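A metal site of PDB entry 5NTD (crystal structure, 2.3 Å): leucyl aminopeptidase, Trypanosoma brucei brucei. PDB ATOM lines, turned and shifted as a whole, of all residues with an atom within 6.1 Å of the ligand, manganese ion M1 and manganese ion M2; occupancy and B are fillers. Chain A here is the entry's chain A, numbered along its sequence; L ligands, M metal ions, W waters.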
ATOM      1  N   LYS A 289      19.262  29.547  31.743  1.00  0.00           N
ATOM      2  CA  LYS A 289      20.699  29.689  31.308  1.00  0.00           C
ATOM      3  C   LYS A 289      20.898  31.101  30.846  1.00  0.00           C
ATOM      4  O   LYS A 289      20.385  31.503  29.801  1.00  0.00           O
ATOM      5  CB  LYS A 289      21.098  28.665  30.188  1.00  0.00           C
ATOM      6  CG  LYS A 289      22.516  28.804  29.670  1.00  0.00           C
ATOM      7  CD  LYS A 289      22.807  27.942  28.431  1.00  0.00           C
ATOM      8  CE  LYS A 289      24.229  28.156  27.859  1.00  0.00           C
ATOM      9  NZ  LYS A 289      24.680  27.388  26.645  1.00  0.00           N
ATOM     10  N   ILE A 291      23.811  32.773  29.899  1.00  0.00           N
ATOM     11  CA  ILE A 291      25.187  32.956  29.382  1.00  0.00           C
ATOM     12  C   ILE A 291      25.163  34.145  28.406  1.00  0.00           C
ATOM     13  O   ILE A 291      24.753  34.029  27.270  1.00  0.00           O
ATOM     14  CB  ILE A 291      25.769  31.692  28.752  1.00  0.00           C
ATOM     15  CG1 ILE A 291      25.824  30.589  29.790  1.00  0.00           C
ATOM     16  CG2 ILE A 291      27.156  31.978  28.192  1.00  0.00           C
ATOM     17  CD1 ILE A 291      26.674  30.874  31.008  1.00  0.00           C
ATOM     18  N   ASP A 294      28.877  33.232  25.022  1.00  0.00           N
ATOM     19  CA  ASP A 294      29.504  31.899  25.081  1.00  0.00           C
ATOM     20  C   ASP A 294      30.652  31.908  24.028  1.00  0.00           C
ATOM     21  O   ASP A 294      30.433  31.582  22.870  1.00  0.00           O
ATOM     22  CB  ASP A 294      28.483  30.774  24.770  1.00  0.00           C
ATOM     23  CG  ASP A 294      29.006  29.349  25.060  1.00  0.00           C
ATOM     24  OD1 ASP A 294      30.166  29.300  25.537  1.00  0.00           O
ATOM     25  OD2 ASP A 294      28.229  28.281  24.951  1.00  0.00           O
ATOM     26  N   GLY A 296      32.998  29.853  24.317  1.00  0.00           N
ATOM     27  CA  GLY A 296      33.491  28.474  24.474  1.00  0.00           C
ATOM     28  C   GLY A 296      34.463  28.241  25.640  1.00  0.00           C
ATOM     29  O   GLY A 296      34.689  27.114  26.059  1.00  0.00           O
ATOM     30  N   LYS A 301      35.340  28.484  20.589  1.00  0.00           N
ATOM     31  CA  LYS A 301      34.546  28.311  19.376  1.00  0.00           C
ATOM     32  C   LYS A 301      35.234  28.973  18.185  1.00  0.00           C
ATOM     33  O   LYS A 301      35.792  30.057  18.328  1.00  0.00           O
ATOM     34  CB  LYS A 301      33.179  28.939  19.505  1.00  0.00           C
ATOM     35  CG  LYS A 301      32.306  28.300  20.549  1.00  0.00           C
ATOM     36  CD  LYS A 301      30.925  28.949  20.549  1.00  0.00           C
ATOM     37  CE  LYS A 301      30.054  28.370  21.634  1.00  0.00           C
ATOM     38  NZ  LYS A 301      29.731  26.957  21.348  1.00  0.00           N
ATOM     39  N   MET A 309      26.236  33.919  19.706  1.00  0.00           N
ATOM     40  CA  MET A 309      26.284  33.453  21.113  1.00  0.00           C
ATOM     41  C   MET A 309      25.877  34.523  22.153  1.00  0.00           C
ATOM     42  O   MET A 309      25.765  34.249  23.321  1.00  0.00           O
ATOM     43  CB  MET A 309      27.617  32.805  21.464  1.00  0.00           C
ATOM     44  CG  MET A 309      27.828  31.492  20.711  1.00  0.00           C
ATOM     45  SD  MET A 309      26.591  30.237  21.150  1.00  0.00           S
ATOM     46  CE  MET A 309      26.191  29.562  19.540  1.00  0.00           C
ATOM     47  N   ASP A 312      22.835  33.372  23.879  1.00  0.00           N
ATOM     48  CA  ASP A 312      23.011  32.253  24.817  1.00  0.00           C
ATOM     49  C   ASP A 312      22.408  32.520  26.193  1.00  0.00           C
ATOM     50  O   ASP A 312      22.490  31.690  27.099  1.00  0.00           O
ATOM     51  CB  ASP A 312      24.505  31.847  24.963  1.00  0.00           C
ATOM     52  CG  ASP A 312      24.690  30.325  25.138  1.00  0.00           C
ATOM     53  OD1 ASP A 312      23.809  29.586  24.671  1.00  0.00           O
ATOM     54  OD2 ASP A 312      25.723  29.852  25.711  1.00  0.00           O
ATOM     55  N   ASN A 344      30.942  33.161  29.568  1.00  0.00           N
ATOM     56  CA  ASN A 344      31.944  32.087  29.336  1.00  0.00           C
ATOM     57  C   ASN A 344      33.091  32.681  28.536  1.00  0.00           C
ATOM     58  O   ASN A 344      33.060  32.725  27.315  1.00  0.00           O
ATOM     59  CB  ASN A 344      31.340  30.894  28.612  1.00  0.00           C
ATOM     60  CG  ASN A 344      32.214  29.635  28.728  1.00  0.00           C
ATOM     61  OD1 ASN A 344      33.076  29.550  29.587  1.00  0.00           O
ATOM     62  ND2 ASN A 344      31.931  28.646  27.894  1.00  0.00           N
ATOM     63  N   ASN A 369      35.138  19.519  28.589  1.00  0.00           N
ATOM     64  CA  ASN A 369      35.012  20.568  27.612  1.00  0.00           C
ATOM     65  C   ASN A 369      34.340  21.782  28.213  1.00  0.00           C
ATOM     66  O   ASN A 369      33.174  21.743  28.598  1.00  0.00           O
ATOM     67  CB  ASN A 369      34.232  20.053  26.402  1.00  0.00           C
ATOM     68  CG  ASN A 369      34.310  20.997  25.216  1.00  0.00           C
ATOM     69  OD1 ASN A 369      34.015  22.187  25.325  1.00  0.00           O
ATOM     70  ND2 ASN A 369      34.689  20.465  24.068  1.00  0.00           N
ATOM     71  N   THR A 370      35.048  22.903  28.198  1.00  0.00           N
ATOM     72  CA  THR A 370      34.560  24.148  28.806  1.00  0.00           C
ATOM     73  C   THR A 370      33.411  24.788  28.065  1.00  0.00           C
ATOM     74  O   THR A 370      32.733  25.657  28.586  1.00  0.00           O
ATOM     75  CB  THR A 370      35.651  25.202  28.931  1.00  0.00           C
ATOM     76  OG1 THR A 370      36.202  25.494  27.654  1.00  0.00           O
ATOM     77  CG2 THR A 370      36.742  24.750  29.896  1.00  0.00           C
ATOM     78  N   ASP A 371      33.219  24.364  26.833  1.00  0.00           N
ATOM     79  CA  ASP A 371      32.109  24.864  25.979  1.00  0.00           C
ATOM     80  C   ASP A 371      30.735  24.174  26.218  1.00  0.00           C
ATOM     81  O   ASP A 371      29.690  24.661  25.712  1.00  0.00           O
ATOM     82  CB  ASP A 371      32.457  24.781  24.509  1.00  0.00           C
ATOM     83  CG  ASP A 371      31.597  25.688  23.648  1.00  0.00           C
ATOM     84  OD1 ASP A 371      30.793  26.546  24.176  1.00  0.00           O
ATOM     85  OD2 ASP A 371      31.678  25.466  22.425  1.00  0.00           O
ATOM     86  N   ALA A 372      30.790  23.148  27.042  1.00  0.00           N
ATOM     87  CA  ALA A 372      29.598  22.574  27.714  1.00  0.00           C
ATOM     88  C   ALA A 372      29.380  23.205  29.119  1.00  0.00           C
ATOM     89  O   ALA A 372      29.331  22.545  30.128  1.00  0.00           O
ATOM     90  CB  ALA A 372      29.675  21.073  27.804  1.00  0.00           C
ATOM     91  N   GLU A 373      29.223  24.503  29.091  1.00  0.00           N
ATOM     92  CA  GLU A 373      29.154  25.363  30.294  1.00  0.00           C
ATOM     93  C   GLU A 373      27.732  25.473  30.847  1.00  0.00           C
ATOM     94  O   GLU A 373      27.516  25.645  32.029  1.00  0.00           O
ATOM     95  CB  GLU A 373      29.688  26.768  29.988  1.00  0.00           C
ATOM     96  CG  GLU A 373      28.730  27.766  29.305  1.00  0.00           C
ATOM     97  CD  GLU A 373      28.320  27.481  27.857  1.00  0.00           C
ATOM     98  OE1 GLU A 373      27.237  28.024  27.416  1.00  0.00           O
ATOM     99  OE2 GLU A 373      29.103  26.811  27.108  1.00  0.00           O
ATOM    100  N   GLY A 374      26.773  25.385  29.944  1.00  0.00           N
ATOM    101  CA  GLY A 374      25.376  25.653  30.275  1.00  0.00           C
ATOM    102  C   GLY A 374      24.840  24.665  31.277  1.00  0.00           C
ATOM    103  O   GLY A 374      24.214  25.042  32.255  1.00  0.00           O
ATOM    104  N   ARG A 375      25.132  23.393  31.041  1.00  0.00           N
ATOM    105  CA  ARG A 375      24.624  22.345  31.893  1.00  0.00           C
ATOM    106  C   ARG A 375      25.215  22.465  33.322  1.00  0.00           C
ATOM    107  O   ARG A 375      24.563  22.154  34.303  1.00  0.00           O
ATOM    108  CB  ARG A 375      24.891  20.983  31.296  1.00  0.00           C
ATOM    109  CG  ARG A 375      26.358  20.566  31.325  1.00  0.00           C
ATOM    110  CD  ARG A 375      26.598  19.395  30.429  1.00  0.00           C
ATOM    111  NE  ARG A 375      26.433  19.776  29.044  1.00  0.00           N
ATOM    112  CZ  ARG A 375      26.341  18.919  28.052  1.00  0.00           C
ATOM    113  NH1 ARG A 375      26.448  17.618  28.281  1.00  0.00           N
ATOM    114  NH2 ARG A 375      26.137  19.342  26.827  1.00  0.00           N
ATOM    115  N   THR A 401      19.483  27.635  26.009  1.00  0.00           N
ATOM    116  CA  THR A 401      19.984  27.511  24.658  1.00  0.00           C
ATOM    117  C   THR A 401      21.170  26.526  24.700  1.00  0.00           C
ATOM    118  O   THR A 401      22.335  26.913  24.601  1.00  0.00           O
ATOM    119  CB  THR A 401      20.432  28.861  24.105  1.00  0.00           C
ATOM    120  OG1 THR A 401      21.261  29.520  25.067  1.00  0.00           O
ATOM    121  CG2 THR A 401      19.236  29.725  23.794  1.00  0.00           C
ATOM    122  N   LEU A 402      20.851  25.257  24.865  1.00  0.00           N
ATOM    123  CA  LEU A 402      21.842  24.330  25.435  1.00  0.00           C
ATOM    124  C   LEU A 402      22.720  23.566  24.451  1.00  0.00           C
ATOM    125  O   LEU A 402      23.880  23.378  24.723  1.00  0.00           O
ATOM    126  CB  LEU A 402      21.185  23.372  26.428  1.00  0.00           C
ATOM    127  CG  LEU A 402      22.163  22.735  27.433  1.00  0.00           C
ATOM    128  CD1 LEU A 402      22.903  23.774  28.255  1.00  0.00           C
ATOM    129  CD2 LEU A 402      21.387  21.823  28.363  1.00  0.00           C
ATOM    130  N   THR A 403      22.130  23.057  23.385  1.00  0.00           N
ATOM    131  CA  THR A 403      22.846  22.171  22.486  1.00  0.00           C
ATOM    132  C   THR A 403      22.597  22.438  21.016  1.00  0.00           C
ATOM    133  O   THR A 403      21.481  22.717  20.622  1.00  0.00           O
ATOM    134  CB  THR A 403      22.505  20.673  22.715  1.00  0.00           C
ATOM    135  OG1 THR A 403      21.160  20.420  22.350  1.00  0.00           O
ATOM    136  CG2 THR A 403      22.722  20.243  24.148  1.00  0.00           C
ATOM    137  N   GLY A 404      23.642  22.266  20.232  1.00  0.00           N
ATOM    138  CA  GLY A 404      23.504  22.209  18.763  1.00  0.00           C
ATOM    139  C   GLY A 404      22.691  21.026  18.311  1.00  0.00           C
ATOM    140  O   GLY A 404      21.946  21.067  17.355  1.00  0.00           O
ATOM    141  N   ALA A 405      22.815  19.945  19.072  1.00  0.00           N
ATOM    142  CA  ALA A 405      21.987  18.741  18.856  1.00  0.00           C
ATOM    143  C   ALA A 405      20.461  19.059  18.794  1.00  0.00           C
ATOM    144  O   ALA A 405      19.727  18.425  18.093  1.00  0.00           O
ATOM    145  CB  ALA A 405      22.247  17.713  19.954  1.00  0.00           C
ATOM    146  N   LEU A 463      30.550  16.052  29.870  1.00  0.00           N
ATOM    147  CA  LEU A 463      30.391  15.743  28.445  1.00  0.00           C
ATOM    148  C   LEU A 463      30.375  14.267  28.185  1.00  0.00           C
ATOM    149  O   LEU A 463      31.162  13.526  28.701  1.00  0.00           O
ATOM    150  CB  LEU A 463      31.508  16.382  27.606  1.00  0.00           C
ATOM    151  CG  LEU A 463      31.293  16.351  26.096  1.00  0.00           C
ATOM    152  CD1 LEU A 463      30.187  17.312  25.681  1.00  0.00           C
ATOM    153  CD2 LEU A 463      32.547  16.718  25.331  1.00  0.00           C
ATOM    154  N   ARG A 467      29.132  11.304  21.577  1.00  0.00           N
ATOM    155  CA  ARG A 467      28.265  12.462  21.303  1.00  0.00           C
ATOM    156  C   ARG A 467      27.113  12.147  20.352  1.00  0.00           C
ATOM    157  O   ARG A 467      26.185  12.930  20.200  1.00  0.00           O
ATOM    158  CB  ARG A 467      29.095  13.613  20.772  1.00  0.00           C
ATOM    159  CG  ARG A 467      30.167  14.034  21.781  1.00  0.00           C
ATOM    160  CD  ARG A 467      29.943  15.359  22.465  1.00  0.00           C
ATOM    161  NE  ARG A 467      29.230  16.386  21.732  1.00  0.00           N
ATOM    162  CZ  ARG A 467      29.808  17.266  20.928  1.00  0.00           C
ATOM    163  NH1 ARG A 467      29.053  18.160  20.319  1.00  0.00           N
ATOM    164  NH2 ARG A 467      31.132  17.218  20.729  1.00  0.00           N
ATOM    165  N   ALA A 497      17.773  26.221  22.041  1.00  0.00           N
ATOM    166  CA  ALA A 497      18.970  26.744  21.297  1.00  0.00           C
ATOM    167  C   ALA A 497      18.619  27.492  20.006  1.00  0.00           C
ATOM    168  O   ALA A 497      19.000  28.626  19.825  1.00  0.00           O
ATOM    169  CB  ALA A 497      19.932  25.634  20.967  1.00  0.00           C
ATOM    170  N   TYR A 498      17.802  26.887  19.185  1.00  0.00           N
ATOM    171  CA  TYR A 498      17.387  27.504  17.914  1.00  0.00           C
ATOM    172  C   TYR A 498      16.063  28.306  17.888  1.00  0.00           C
ATOM    173  O   TYR A 498      15.968  29.307  17.190  1.00  0.00           O
ATOM    174  CB  TYR A 498      17.388  26.455  16.814  1.00  0.00           C
ATOM    175  CG  TYR A 498      18.788  26.020  16.467  1.00  0.00           C
ATOM    176  CD1 TYR A 498      19.436  25.033  17.198  1.00  0.00           C
ATOM    177  CD2 TYR A 498      19.506  26.660  15.429  1.00  0.00           C
ATOM    178  CE1 TYR A 498      20.721  24.652  16.890  1.00  0.00           C
ATOM    179  CE2 TYR A 498      20.796  26.299  15.126  1.00  0.00           C
ATOM    180  CZ  TYR A 498      21.406  25.291  15.852  1.00  0.00           C
ATOM    181  OH  TYR A 498      22.694  24.916  15.550  1.00  0.00           O
ATOM    182  N   PHE A 501      15.784  32.370  18.045  1.00  0.00           N
ATOM    183  CA  PHE A 501      16.196  33.275  16.987  1.00  0.00           C
ATOM    184  C   PHE A 501      15.797  32.813  15.608  1.00  0.00           C
ATOM    185  O   PHE A 501      15.539  31.665  15.369  1.00  0.00           O
ATOM    186  CB  PHE A 501      17.694  33.570  17.062  1.00  0.00           C
ATOM    187  CG  PHE A 501      18.552  32.461  16.494  1.00  0.00           C
ATOM    188  CD1 PHE A 501      18.901  31.353  17.262  1.00  0.00           C
ATOM    189  CD2 PHE A 501      19.045  32.551  15.188  1.00  0.00           C
ATOM    190  CE1 PHE A 501      19.701  30.353  16.754  1.00  0.00           C
ATOM    191  CE2 PHE A 501      19.864  31.548  14.676  1.00  0.00           C
ATOM    192  CZ  PHE A 501      20.172  30.434  15.453  1.00  0.00           C
HETATM  193  N1  LIG L   1      25.489  27.560  23.950  1.00  0.00           N
HETATM  194  C1  LIG L   1      25.904  26.448  23.127  1.00  0.00           C
HETATM  195  C2  LIG L   1      24.780  25.737  22.344  1.00  0.00           C
HETATM  196  C3  LIG L   1      24.331  26.275  20.989  1.00  0.00           C
HETATM  197  C4  LIG L   1      23.452  27.335  20.896  1.00  0.00           C
HETATM  198  C5  LIG L   1      24.723  25.651  19.798  1.00  0.00           C
HETATM  199  C6  LIG L   1      23.016  27.771  19.651  1.00  0.00           C
HETATM  200  C7  LIG L   1      24.295  26.121  18.557  1.00  0.00           C
HETATM  201  C8  LIG L   1      23.431  27.200  18.467  1.00  0.00           C
HETATM  202  C9  LIG L   1      26.528  25.497  24.146  1.00  0.00           C
HETATM  203  O1  LIG L   1      27.133  26.284  25.204  1.00  0.00           O
HETATM  204  C10 LIG L   1      27.631  24.760  23.486  1.00  0.00           C
HETATM  205  O2  LIG L   1      28.715  25.341  23.550  1.00  0.00           O
HETATM  206  N2  LIG L   1      27.305  23.581  22.967  1.00  0.00           N
HETATM  207  C11 LIG L   1      28.206  22.667  22.316  1.00  0.00           C
HETATM  208  C12 LIG L   1      28.906  21.736  23.324  1.00  0.00           C
HETATM  209  C13 LIG L   1      30.131  21.008  22.788  1.00  0.00           C
HETATM  210  C14 LIG L   1      31.137  21.867  22.003  1.00  0.00           C
HETATM  211  C15 LIG L   1      30.889  20.366  23.931  1.00  0.00           C
HETATM  212  C16 LIG L   1      27.468  21.816  21.327  1.00  0.00           C
HETATM  213  O3  LIG L   1      26.266  21.640  21.536  1.00  0.00           O
HETATM  214  O4  LIG L   1      28.067  21.320  20.338  1.00  0.00           O
HETATM  215 MN    MN M   1      26.369  28.034  25.698  1.00  0.00          MN
HETATM  216 MN    MN M   2      29.097  26.465  25.133  1.00  0.00          MN
HETATM  217  O   HOH W   1      25.221  19.228  20.704  1.00  0.00           O
HETATM  218  O   HOH W   2      22.932  30.336  21.990  1.00  0.00           O
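Manganese ion M2 is bound by OD1 of Asp 371, O1 of the ligand, O2 of the ligand, O of Asp 371, OE2 of Glu 373 and OD2 of Asp 294. Manganese ion M2 has six donor atoms within binding distance.
NZ of Lys 301 lies close to O2 of the ligand, 2.9 Å away. The backbone NH of Gly 404 sits at hydrogen-bond distance from an oxygen (O3) of the ligand. A nitrogen (N1) of the ligand sits close to the backbone carbonyl oxygen (O) of Thr 401 (3.3 Å). NH1 of Arg 467 lies within salt-bridge range of O4 of the ligand (3.3 Å).
The nearest printed residue that does not touch manganese ion M1 is Thr 401 (4.3 Å).
OD1 of Asp 312 is in hydrogen-bond range of OG1 of Thr 401 (2.6 Å). The backbone carbonyl oxygen of Asp 312 is in hydrogen-bond range of the backbone NH of Ile 291. The side-chain carboxylate (OD2) of Asp 371 is in salt-bridge range of the side-chain amino group (NZ) of Lys 301, at 2.7 Å. N of Asp 371 sits at hydrogen-bond distance from OD1 of Asn 369. O of Gly 296 is in hydrogen-bond range of N of Asp 371, 3.2 Å away. The side-chain amide nitrogen (ND2) of Asn 344 sits at hydrogen-bond distance from the side-chain carboxylate (OD1) of Asp 294 (3.0 Å). OD1 of Asp 294 is in hydrogen-bond range of N of Gly 296 (3.1 Å). The side-chain amino group of Lys 289 lies close to the backbone carbonyl oxygen of Thr 401, at 3.1 Å.
CE of Met 309 touches C6 of the ligand, at 3.6 Å. Asn 369 touches the ligand (CG to C15, 3.7 Å). Leu 402 touches the ligand (O to C9, 3.4 Å). Thr 403 touches the ligand (CA to O3, 3.6 Å). Leu 463 touches the ligand. CB of Ala 497 touches C4 of the ligand, 3.9 Å away. Tyr 498 touches the ligand (OH to C7, 3.6 Å). Hydrophobic or aromatic side chains within 4 Å of the ligand: Met 309, Leu 463, Ala 497 and Tyr 498. Of the 25 residues printed, 16 come within 4 Å of the ligand. The nearest printed residue that does not touch the ligand is Ala 372 (4.1 Å).
Water W1 lies within hydrogen-bond range of O3 of the ligand, N of Ala 405 and N of Gly 404. Water W2 bridges the side-chain carboxylate of Asp 312 and the side-chain sulfur of Met 309.
Manganese ion M1 is bound by OE1 of Glu 373 (1.9 Å), OD2 of Asp 312 (1.9 Å), O1 of the ligand (2.0 Å), N1 of the ligand (2.0 Å), OD2 of Asp 294 (2.0 Å) and NZ of Lys 289 (2.0 Å). Manganese ion M1 has six donor atoms within binding distance.
Lys 301 touches manganese ion M2. Four residues have an atom within 4 Å of manganese ion M2: Asp 294, Lys 301, Asp 371 and Glu 373. The nearest printed residue that does not touch manganese ion M2 is Ala 372 (4.2 Å).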
